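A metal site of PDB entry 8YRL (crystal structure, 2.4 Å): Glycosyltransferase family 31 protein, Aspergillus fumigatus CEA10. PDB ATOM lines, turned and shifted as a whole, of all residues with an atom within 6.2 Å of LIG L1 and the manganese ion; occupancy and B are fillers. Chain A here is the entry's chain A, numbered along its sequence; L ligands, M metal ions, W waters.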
ATOM      1  N   LEU A 130     -26.608  24.292 -37.426  1.00  0.00           N
ATOM      2  CA  LEU A 130     -25.874  23.572 -36.407  1.00  0.00           C
ATOM      3  C   LEU A 130     -24.865  22.636 -37.052  1.00  0.00           C
ATOM      4  O   LEU A 130     -25.149  22.012 -38.082  1.00  0.00           O
ATOM      5  CB  LEU A 130     -26.819  22.778 -35.499  1.00  0.00           C
ATOM      6  CG  LEU A 130     -27.516  23.551 -34.385  1.00  0.00           C
ATOM      7  CD1 LEU A 130     -28.661  22.747 -33.790  1.00  0.00           C
ATOM      8  CD2 LEU A 130     -26.522  23.929 -33.312  1.00  0.00           C
ATOM      9  N   ALA A 131     -23.690  22.535 -36.438  1.00  0.00           N
ATOM     10  CA  ALA A 131     -22.679  21.541 -36.792  1.00  0.00           C
ATOM     11  C   ALA A 131     -22.523  20.630 -35.579  1.00  0.00           C
ATOM     12  O   ALA A 131     -21.778  20.956 -34.647  1.00  0.00           O
ATOM     13  CB  ALA A 131     -21.359  22.208 -37.180  1.00  0.00           C
ATOM     14  N   THR A 132     -23.237  19.517 -35.587  1.00  0.00           N
ATOM     15  CA  THR A 132     -23.262  18.595 -34.454  1.00  0.00           C
ATOM     16  C   THR A 132     -23.704  17.231 -34.955  1.00  0.00           C
ATOM     17  O   THR A 132     -23.770  16.985 -36.168  1.00  0.00           O
ATOM     18  CB  THR A 132     -24.166  19.130 -33.342  1.00  0.00           C
ATOM     19  OG1 THR A 132     -24.049  18.298 -32.178  1.00  0.00           O
ATOM     20  CG2 THR A 132     -25.618  19.164 -33.794  1.00  0.00           C
ATOM     21  N   THR A 133     -24.011  16.331 -34.026  1.00  0.00           N
ATOM     22  CA  THR A 133     -24.436  14.981 -34.351  1.00  0.00           C
ATOM     23  C   THR A 133     -25.852  14.740 -33.819  1.00  0.00           C
ATOM     24  O   THR A 133     -26.352  15.481 -32.975  1.00  0.00           O
ATOM     25  CB  THR A 133     -23.485  13.928 -33.773  1.00  0.00           C
ATOM     26  OG1 THR A 133     -23.527  13.983 -32.338  1.00  0.00           O
ATOM     27  CG2 THR A 133     -22.058  14.193 -34.240  1.00  0.00           C
ATOM     28  N   ARG A 136     -25.763  14.125 -30.062  1.00  0.00           N
ATOM     29  CA  ARG A 136     -25.721  15.327 -29.233  1.00  0.00           C
ATOM     30  C   ARG A 136     -27.067  16.035 -29.210  1.00  0.00           C
ATOM     31  O   ARG A 136     -27.460  16.614 -28.191  1.00  0.00           O
ATOM     32  CB  ARG A 136     -24.626  16.278 -29.732  1.00  0.00           C
ATOM     33  CG  ARG A 136     -23.207  15.749 -29.543  1.00  0.00           C
ATOM     34  CD  ARG A 136     -22.180  16.759 -30.024  1.00  0.00           C
ATOM     35  NE  ARG A 136     -22.266  18.013 -29.282  1.00  0.00           N
ATOM     36  CZ  ARG A 136     -21.632  18.243 -28.140  1.00  0.00           C
ATOM     37  NH1 ARG A 136     -20.846  17.339 -27.579  1.00  0.00           N
ATOM     38  NH2 ARG A 136     -21.790  19.426 -27.536  1.00  0.00           N
ATOM     39  N   PHE A 189     -15.833  19.154 -37.848  1.00  0.00           N
ATOM     40  CA  PHE A 189     -16.700  20.034 -37.059  1.00  0.00           C
ATOM     41  C   PHE A 189     -16.332  21.500 -37.238  1.00  0.00           C
ATOM     42  O   PHE A 189     -17.210  22.365 -37.316  1.00  0.00           O
ATOM     43  CB  PHE A 189     -16.654  19.637 -35.586  1.00  0.00           C
ATOM     44  CG  PHE A 189     -17.161  20.715 -34.667  1.00  0.00           C
ATOM     45  CD1 PHE A 189     -18.524  20.932 -34.524  1.00  0.00           C
ATOM     46  CD2 PHE A 189     -16.282  21.502 -33.943  1.00  0.00           C
ATOM     47  CE1 PHE A 189     -18.998  21.917 -33.687  1.00  0.00           C
ATOM     48  CE2 PHE A 189     -16.753  22.492 -33.098  1.00  0.00           C
ATOM     49  CZ  PHE A 189     -18.112  22.698 -32.974  1.00  0.00           C
ATOM     50  N   ARG A 192     -17.330  22.343 -40.824  1.00  0.00           N
ATOM     51  CA  ARG A 192     -18.770  22.238 -41.006  1.00  0.00           C
ATOM     52  C   ARG A 192     -19.495  23.457 -40.460  1.00  0.00           C
ATOM     53  O   ARG A 192     -20.573  23.815 -40.948  1.00  0.00           O
ATOM     54  CB  ARG A 192     -19.298  20.964 -40.347  1.00  0.00           C
ATOM     55  CG  ARG A 192     -19.506  19.809 -41.317  1.00  0.00           C
ATOM     56  CD  ARG A 192     -19.557  18.470 -40.598  1.00  0.00           C
ATOM     57  NE  ARG A 192     -20.434  18.497 -39.432  1.00  0.00           N
ATOM     58  CZ  ARG A 192     -20.152  17.883 -38.289  1.00  0.00           C
ATOM     59  NH1 ARG A 192     -19.034  17.200 -38.121  1.00  0.00           N
ATOM     60  NH2 ARG A 192     -21.032  17.956 -37.288  1.00  0.00           N
ATOM     61  N   ILE A 217     -25.279  28.836 -34.509  1.00  0.00           N
ATOM     62  CA  ILE A 217     -25.501  28.517 -33.108  1.00  0.00           C
ATOM     63  C   ILE A 217     -24.734  27.255 -32.745  1.00  0.00           C
ATOM     64  O   ILE A 217     -24.431  26.416 -33.582  1.00  0.00           O
ATOM     65  CB  ILE A 217     -26.991  28.330 -32.778  1.00  0.00           C
ATOM     66  CG1 ILE A 217     -27.661  27.468 -33.848  1.00  0.00           C
ATOM     67  CG2 ILE A 217     -27.689  29.674 -32.627  1.00  0.00           C
ATOM     68  CD1 ILE A 217     -28.958  26.839 -33.407  1.00  0.00           C
ATOM     69  N   ASP A 218     -24.415  27.143 -31.451  1.00  0.00           N
ATOM     70  CA  ASP A 218     -23.964  25.898 -30.860  1.00  0.00           C
ATOM     71  C   ASP A 218     -25.172  25.100 -30.387  1.00  0.00           C
ATOM     72  O   ASP A 218     -26.256  25.626 -30.188  1.00  0.00           O
ATOM     73  CB  ASP A 218     -23.010  26.160 -29.688  1.00  0.00           C
ATOM     74  CG  ASP A 218     -21.595  26.447 -30.138  1.00  0.00           C
ATOM     75  OD1 ASP A 218     -21.406  26.996 -31.243  1.00  0.00           O
ATOM     76  OD2 ASP A 218     -20.659  26.121 -29.377  1.00  0.00           O
ATOM     77  N   ASP A 219     -24.960  23.783 -30.205  1.00  0.00           N
ATOM     78  CA  ASP A 219     -26.056  22.965 -29.691  1.00  0.00           C
ATOM     79  C   ASP A 219     -26.357  23.258 -28.224  1.00  0.00           C
ATOM     80  O   ASP A 219     -27.412  22.832 -27.741  1.00  0.00           O
ATOM     81  CB  ASP A 219     -25.746  21.474 -29.882  1.00  0.00           C
ATOM     82  CG  ASP A 219     -24.403  21.066 -29.312  1.00  0.00           C
ATOM     83  OD1 ASP A 219     -23.825  21.823 -28.509  1.00  0.00           O
ATOM     84  OD2 ASP A 219     -23.929  19.969 -29.663  1.00  0.00           O
ATOM     85  N   ASP A 220     -25.468  23.964 -27.522  1.00  0.00           N
ATOM     86  CA  ASP A 220     -25.724  24.411 -26.164  1.00  0.00           C
ATOM     87  C   ASP A 220     -25.977  25.909 -26.080  1.00  0.00           C
ATOM     88  O   ASP A 220     -25.825  26.505 -25.011  1.00  0.00           O
ATOM     89  CB  ASP A 220     -24.571  24.012 -25.243  1.00  0.00           C
ATOM     90  CG  ASP A 220     -23.267  24.679 -25.612  1.00  0.00           C
ATOM     91  OD1 ASP A 220     -23.065  24.990 -26.799  1.00  0.00           O
ATOM     92  OD2 ASP A 220     -22.435  24.896 -24.704  1.00  0.00           O
ATOM     93  N   THR A 221     -26.354  26.542 -27.198  1.00  0.00           N
ATOM     94  CA  THR A 221     -26.806  27.924 -27.182  1.00  0.00           C
ATOM     95  C   THR A 221     -28.277  27.929 -26.769  1.00  0.00           C
ATOM     96  O   THR A 221     -29.142  27.457 -27.521  1.00  0.00           O
ATOM     97  CB  THR A 221     -26.612  28.582 -28.548  1.00  0.00           C
ATOM     98  OG1 THR A 221     -25.218  28.699 -28.830  1.00  0.00           O
ATOM     99  CG2 THR A 221     -27.237  29.972 -28.556  1.00  0.00           C
ATOM    100  N   GLY A 264     -20.866  30.820 -29.356  1.00  0.00           N
ATOM    101  CA  GLY A 264     -21.625  30.261 -28.248  1.00  0.00           C
ATOM    102  C   GLY A 264     -22.830  31.098 -27.870  1.00  0.00           C
ATOM    103  O   GLY A 264     -23.898  30.570 -27.554  1.00  0.00           O
ATOM    104  N   GLN A 316     -21.750  34.532 -24.043  1.00  0.00           N
ATOM    105  CA  GLN A 316     -20.950  33.373 -24.388  1.00  0.00           C
ATOM    106  C   GLN A 316     -20.610  32.532 -23.172  1.00  0.00           C
ATOM    107  O   GLN A 316     -20.487  31.305 -23.276  1.00  0.00           O
ATOM    108  CB  GLN A 316     -19.674  33.832 -25.101  1.00  0.00           C
ATOM    109  CG  GLN A 316     -18.544  32.814 -25.107  1.00  0.00           C
ATOM    110  CD  GLN A 316     -18.698  31.779 -26.207  1.00  0.00           C
ATOM    111  OE1 GLN A 316     -19.258  32.059 -27.262  1.00  0.00           O
ATOM    112  NE2 GLN A 316     -18.202  30.568 -25.948  1.00  0.00           N
ATOM    113  N   ASP A 318     -17.757  32.561 -21.216  1.00  0.00           N
ATOM    114  CA  ASP A 318     -16.369  32.078 -21.218  1.00  0.00           C
ATOM    115  C   ASP A 318     -15.820  32.156 -19.799  1.00  0.00           C
ATOM    116  O   ASP A 318     -14.911  32.930 -19.472  1.00  0.00           O
ATOM    117  CB  ASP A 318     -15.527  32.874 -22.196  1.00  0.00           C
ATOM    118  CG  ASP A 318     -15.572  32.313 -23.608  1.00  0.00           C
ATOM    119  OD1 ASP A 318     -15.999  31.146 -23.766  1.00  0.00           O
ATOM    120  OD2 ASP A 318     -15.182  33.019 -24.550  1.00  0.00           O
ATOM    121  N   HIS A 337     -24.905  29.914 -22.526  1.00  0.00           N
ATOM    122  CA  HIS A 337     -23.951  29.024 -23.175  1.00  0.00           C
ATOM    123  C   HIS A 337     -23.062  28.386 -22.114  1.00  0.00           C
ATOM    124  O   HIS A 337     -22.977  28.884 -20.980  1.00  0.00           O
ATOM    125  CB  HIS A 337     -23.121  29.788 -24.214  1.00  0.00           C
ATOM    126  CG  HIS A 337     -22.203  28.920 -25.016  1.00  0.00           C
ATOM    127  ND1 HIS A 337     -20.831  29.087 -25.019  1.00  0.00           N
ATOM    128  CD2 HIS A 337     -22.457  27.877 -25.850  1.00  0.00           C
ATOM    129  CE1 HIS A 337     -20.278  28.184 -25.821  1.00  0.00           C
ATOM    130  NE2 HIS A 337     -21.240  27.438 -26.333  1.00  0.00           N
ATOM    131  N   HIS A 338     -22.416  27.286 -22.491  1.00  0.00           N
ATOM    132  CA  HIS A 338     -21.422  26.578 -21.694  1.00  0.00           C
ATOM    133  C   HIS A 338     -21.996  25.946 -20.426  1.00  0.00           C
ATOM    134  O   HIS A 338     -21.236  25.504 -19.563  1.00  0.00           O
ATOM    135  CB  HIS A 338     -20.250  27.483 -21.307  1.00  0.00           C
ATOM    136  CG  HIS A 338     -19.181  27.576 -22.359  1.00  0.00           C
ATOM    137  ND1 HIS A 338     -18.383  28.688 -22.511  1.00  0.00           N
ATOM    138  CD2 HIS A 338     -18.788  26.695 -23.303  1.00  0.00           C
ATOM    139  CE1 HIS A 338     -17.537  28.485 -23.503  1.00  0.00           C
ATOM    140  NE2 HIS A 338     -17.766  27.290 -24.005  1.00  0.00           N
ATOM    141  N   ASN A 340     -23.375  23.163 -19.909  1.00  0.00           N
ATOM    142  CA  ASN A 340     -23.236  21.719 -19.824  1.00  0.00           C
ATOM    143  C   ASN A 340     -21.812  21.280 -20.159  1.00  0.00           C
ATOM    144  O   ASN A 340     -21.602  20.179 -20.671  1.00  0.00           O
ATOM    145  CB  ASN A 340     -24.252  21.021 -20.734  1.00  0.00           C
ATOM    146  CG  ASN A 340     -24.559  19.599 -20.280  1.00  0.00           C
ATOM    147  OD1 ASN A 340     -24.768  18.707 -21.102  1.00  0.00           O
ATOM    148  ND2 ASN A 340     -24.574  19.378 -18.971  1.00  0.00           N
ATOM    149  N   SER A 341     -20.825  22.137 -19.880  1.00  0.00           N
ATOM    150  CA  SER A 341     -19.442  21.843 -20.204  1.00  0.00           C
ATOM    151  C   SER A 341     -18.479  22.631 -19.322  1.00  0.00           C
ATOM    152  O   SER A 341     -17.925  22.083 -18.362  1.00  0.00           O
ATOM    153  CB  SER A 341     -19.162  22.137 -21.685  1.00  0.00           C
ATOM    154  OG  SER A 341     -19.309  23.519 -21.949  1.00  0.00           O
ATOM    155  N   TRP A 342     -18.280  23.917 -19.640  1.00  0.00           N
ATOM    156  CA  TRP A 342     -17.401  24.749 -18.833  1.00  0.00           C
ATOM    157  C   TRP A 342     -17.915  24.866 -17.398  1.00  0.00           C
ATOM    158  O   TRP A 342     -17.129  24.848 -16.445  1.00  0.00           O
ATOM    159  CB  TRP A 342     -17.256  26.129 -19.466  1.00  0.00           C
ATOM    160  CG  TRP A 342     -16.284  26.168 -20.607  1.00  0.00           C
ATOM    161  CD1 TRP A 342     -16.064  25.185 -21.529  1.00  0.00           C
ATOM    162  CD2 TRP A 342     -15.385  27.233 -20.939  1.00  0.00           C
ATOM    163  NE1 TRP A 342     -15.091  25.569 -22.412  1.00  0.00           N
ATOM    164  CE2 TRP A 342     -14.653  26.820 -22.076  1.00  0.00           C
ATOM    165  CE3 TRP A 342     -15.132  28.494 -20.397  1.00  0.00           C
ATOM    166  CZ2 TRP A 342     -13.684  27.636 -22.672  1.00  0.00           C
ATOM    167  CZ3 TRP A 342     -14.165  29.291 -20.983  1.00  0.00           C
ATOM    168  CH2 TRP A 342     -13.465  28.863 -22.111  1.00  0.00           C
HETATM  169  N1  LIG L   1     -19.754  20.609 -30.478  1.00  0.00           N
HETATM  170  C1  LIG L   1     -20.501  20.149 -31.552  1.00  0.00           C
HETATM  171  N2  LIG L   1     -21.531  20.972 -31.932  1.00  0.00           N
HETATM  172  C2  LIG L   1     -21.889  22.178 -31.349  1.00  0.00           C
HETATM  173  C3  LIG L   1     -21.074  22.573 -30.242  1.00  0.00           C
HETATM  174  C4  LIG L   1     -20.055  21.788 -29.854  1.00  0.00           C
HETATM  175  O1  LIG L   1     -20.256  19.101 -32.129  1.00  0.00           O
HETATM  176  O2  LIG L   1     -22.862  22.809 -31.805  1.00  0.00           O
HETATM  177  C5  LIG L   1     -18.636  19.773 -30.028  1.00  0.00           C
HETATM  178  C6  LIG L   1     -17.286  20.172 -30.654  1.00  0.00           C
HETATM  179  O3  LIG L   1     -16.482  19.023 -30.875  1.00  0.00           O
HETATM  180  C7  LIG L   1     -16.697  21.082 -29.567  1.00  0.00           C
HETATM  181  C8  LIG L   1     -17.184  20.402 -28.294  1.00  0.00           C
HETATM  182  O4  LIG L   1     -18.508  19.917 -28.619  1.00  0.00           O
HETATM  183  O5  LIG L   1     -15.278  21.120 -29.614  1.00  0.00           O
HETATM  184  C9  LIG L   1     -17.249  21.298 -27.076  1.00  0.00           C
HETATM  185  O6  LIG L   1     -18.116  22.420 -27.352  1.00  0.00           O
HETATM  186  P1  LIG L   1     -18.751  23.258 -26.176  1.00  0.00           P
HETATM  187  O7  LIG L   1     -19.960  23.925 -26.718  1.00  0.00           O
HETATM  188  O8  LIG L   1     -18.932  22.409 -24.929  1.00  0.00           O
HETATM  189  O9  LIG L   1     -17.652  24.349 -25.812  1.00  0.00           O
HETATM  190  P2  LIG L   1     -17.100  25.435 -26.834  1.00  0.00           P
HETATM  191  O10 LIG L   1     -16.330  24.816 -27.949  1.00  0.00           O
HETATM  192  O11 LIG L   1     -16.274  26.355 -25.935  1.00  0.00           O
HETATM  193  O12 LIG L   1     -18.376  26.161 -27.275  1.00  0.00           O
HETATM  194  C1  LG2 L   2     -13.171  30.773 -30.880  1.00  0.00           C
HETATM  195  C2  LG2 L   2     -14.117  30.983 -29.677  1.00  0.00           C
HETATM  196  C3  LG2 L   2     -13.340  30.518 -28.415  1.00  0.00           C
HETATM  197  C4  LG2 L   2     -14.327  30.376 -27.215  1.00  0.00           C
HETATM  198  C5  LG2 L   2     -13.962  28.968 -26.662  1.00  0.00           C
HETATM  199  O1  LG2 L   2     -13.517  31.686 -31.858  1.00  0.00           O
HETATM  200  O2  LG2 L   2     -15.230  30.144 -29.811  1.00  0.00           O
HETATM  201  O3  LG2 L   2     -12.740  29.262 -28.647  1.00  0.00           O
HETATM  202  O4  LG2 L   2     -14.008  31.379 -26.302  1.00  0.00           O
HETATM  203  C6  LG2 L   2     -12.619  28.647 -27.396  1.00  0.00           C
HETATM  204  O5  LG2 L   2     -14.934  28.097 -27.153  1.00  0.00           O
HETATM  205  O6  LG2 L   2     -11.614  29.310 -26.738  1.00  0.00           O
HETATM  206 MN    MN M   1     -20.793  25.607 -27.217  1.00  0.00          MN
HETATM  207  O   HOH W   1     -13.935  24.815 -25.511  1.00  0.00           O
HETATM  208  O   HOH W   2     -16.131  22.262 -23.635  1.00  0.00           O
HETATM  209  O   HOH W   3     -18.137  24.909 -30.070  1.00  0.00           O
HETATM  210  O   HOH W   4     -18.271  28.605 -28.722  1.00  0.00           O
HETATM  211  O   HOH W   5     -22.929  23.995 -34.407  1.00  0.00           O
HETATM  212  O   HOH W   6     -20.734  19.982 -24.809  1.00  0.00           O
HETATM  213  O   HOH W   7     -22.248  21.839 -26.465  1.00  0.00           O
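NE2 of His 338 is in hydrogen-bond range of O11 of LIG L1, 2.6 Å away.
A nitrogen (N2) of LIG L1 sits at hydrogen-bond distance from the backbone carbonyl oxygen (O) of Ala 131 (2.7 Å).
N of Asp 219 lies within hydrogen-bond range of O2 of LIG L1, at 2.8 Å.
The side-chain carboxylate (OD2) of Asp 219 lies close to a nitrogen (N2) of LIG L1 (3.5 Å).
The side-chain hydroxyl (OG) of Ser 341 sits at hydrogen-bond distance from an oxygen (O8) of LIG L1, at 3.2 Å.
The guanidinium group of Arg 136 lies within hydrogen-bond range of an oxygen (O4) of LIG L1 (3.5 Å).
OD2 of Asp 318 lies within hydrogen-bond range of O4 of LG2 L2 (2.7 Å).
An oxygen (O5) of LG2 L2 is in hydrogen-bond range of an oxygen (O11) of LIG L1, at 2.5 Å.
ND1 of His 337 is in hydrogen-bond range of O of Gln 316 (2.8 Å).
N of Asp 218 sits at hydrogen-bond distance from OG1 of Thr 221 (3.2 Å).
The backbone NH of His 338 lies within hydrogen-bond range of the side-chain carboxylate of Asp 220, 3.3 Å away.
A ring nitrogen (ND1) of His 338 lies within hydrogen-bond range of the backbone carbonyl oxygen (O) of Gln 316.
OD2 of Asp 219 is in salt-bridge range of NE of Arg 136, 2.6 Å away.
The side-chain carboxylate (OD2) of Asp 219 lies within hydrogen-bond range of the side-chain hydroxyl (OG1) of Thr 132 (3.0 Å).
The backbone NH of Arg 136 is in hydrogen-bond range of the side-chain hydroxyl of Thr 133 (3.2 Å).
The backbone carbonyl oxygen of Thr 132 sits at hydrogen-bond distance from the guanidinium group of Arg 192 (3.1 Å).
Thr 132 touches LIG L1.
Phe 189 touches LIG L1.
Trp 342 touches LIG L1.
Hydrophobic or aromatic side chains that line LIG L1: Phe 189, His 337 and His 338.
Of the 20 residues printed, 11 come within 4 Å of LIG L1.
The nearest printed residue that does not touch the manganese ion is His 338 (4.5 Å).
The manganese ion is bound by an oxygen (O7) of LIG L1, a ring nitrogen (NE2) of His 337, the side-chain carboxylate (OD2) of Asp 218, the side-chain carboxylate (OD1) of Asp 220 and an oxygen (O12) of LIG L1.
Water W1 bridges an oxygen (O11) of LIG L1 and the indole nitrogen of Trp 342.
Water W4 lies within hydrogen-bond range of the side-chain amide nitrogen (NE2) of Gln 316 and the backbone NH (N) of Gly 264.
Water W5 lies within hydrogen-bond range of N of Ala 131 (2.6 Å), O2 of LIG L1 (2.9 Å) and O of Ile 217 (3.0 Å).
Water W6 lies within hydrogen-bond range of NH2 of Arg 136 (3.0 Å) and O8 of LIG L1 (3.0 Å).
Water W7 bridges the side-chain carboxylate (OD1) of Asp 219 and the guanidinium group (NH2) of Arg 136.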
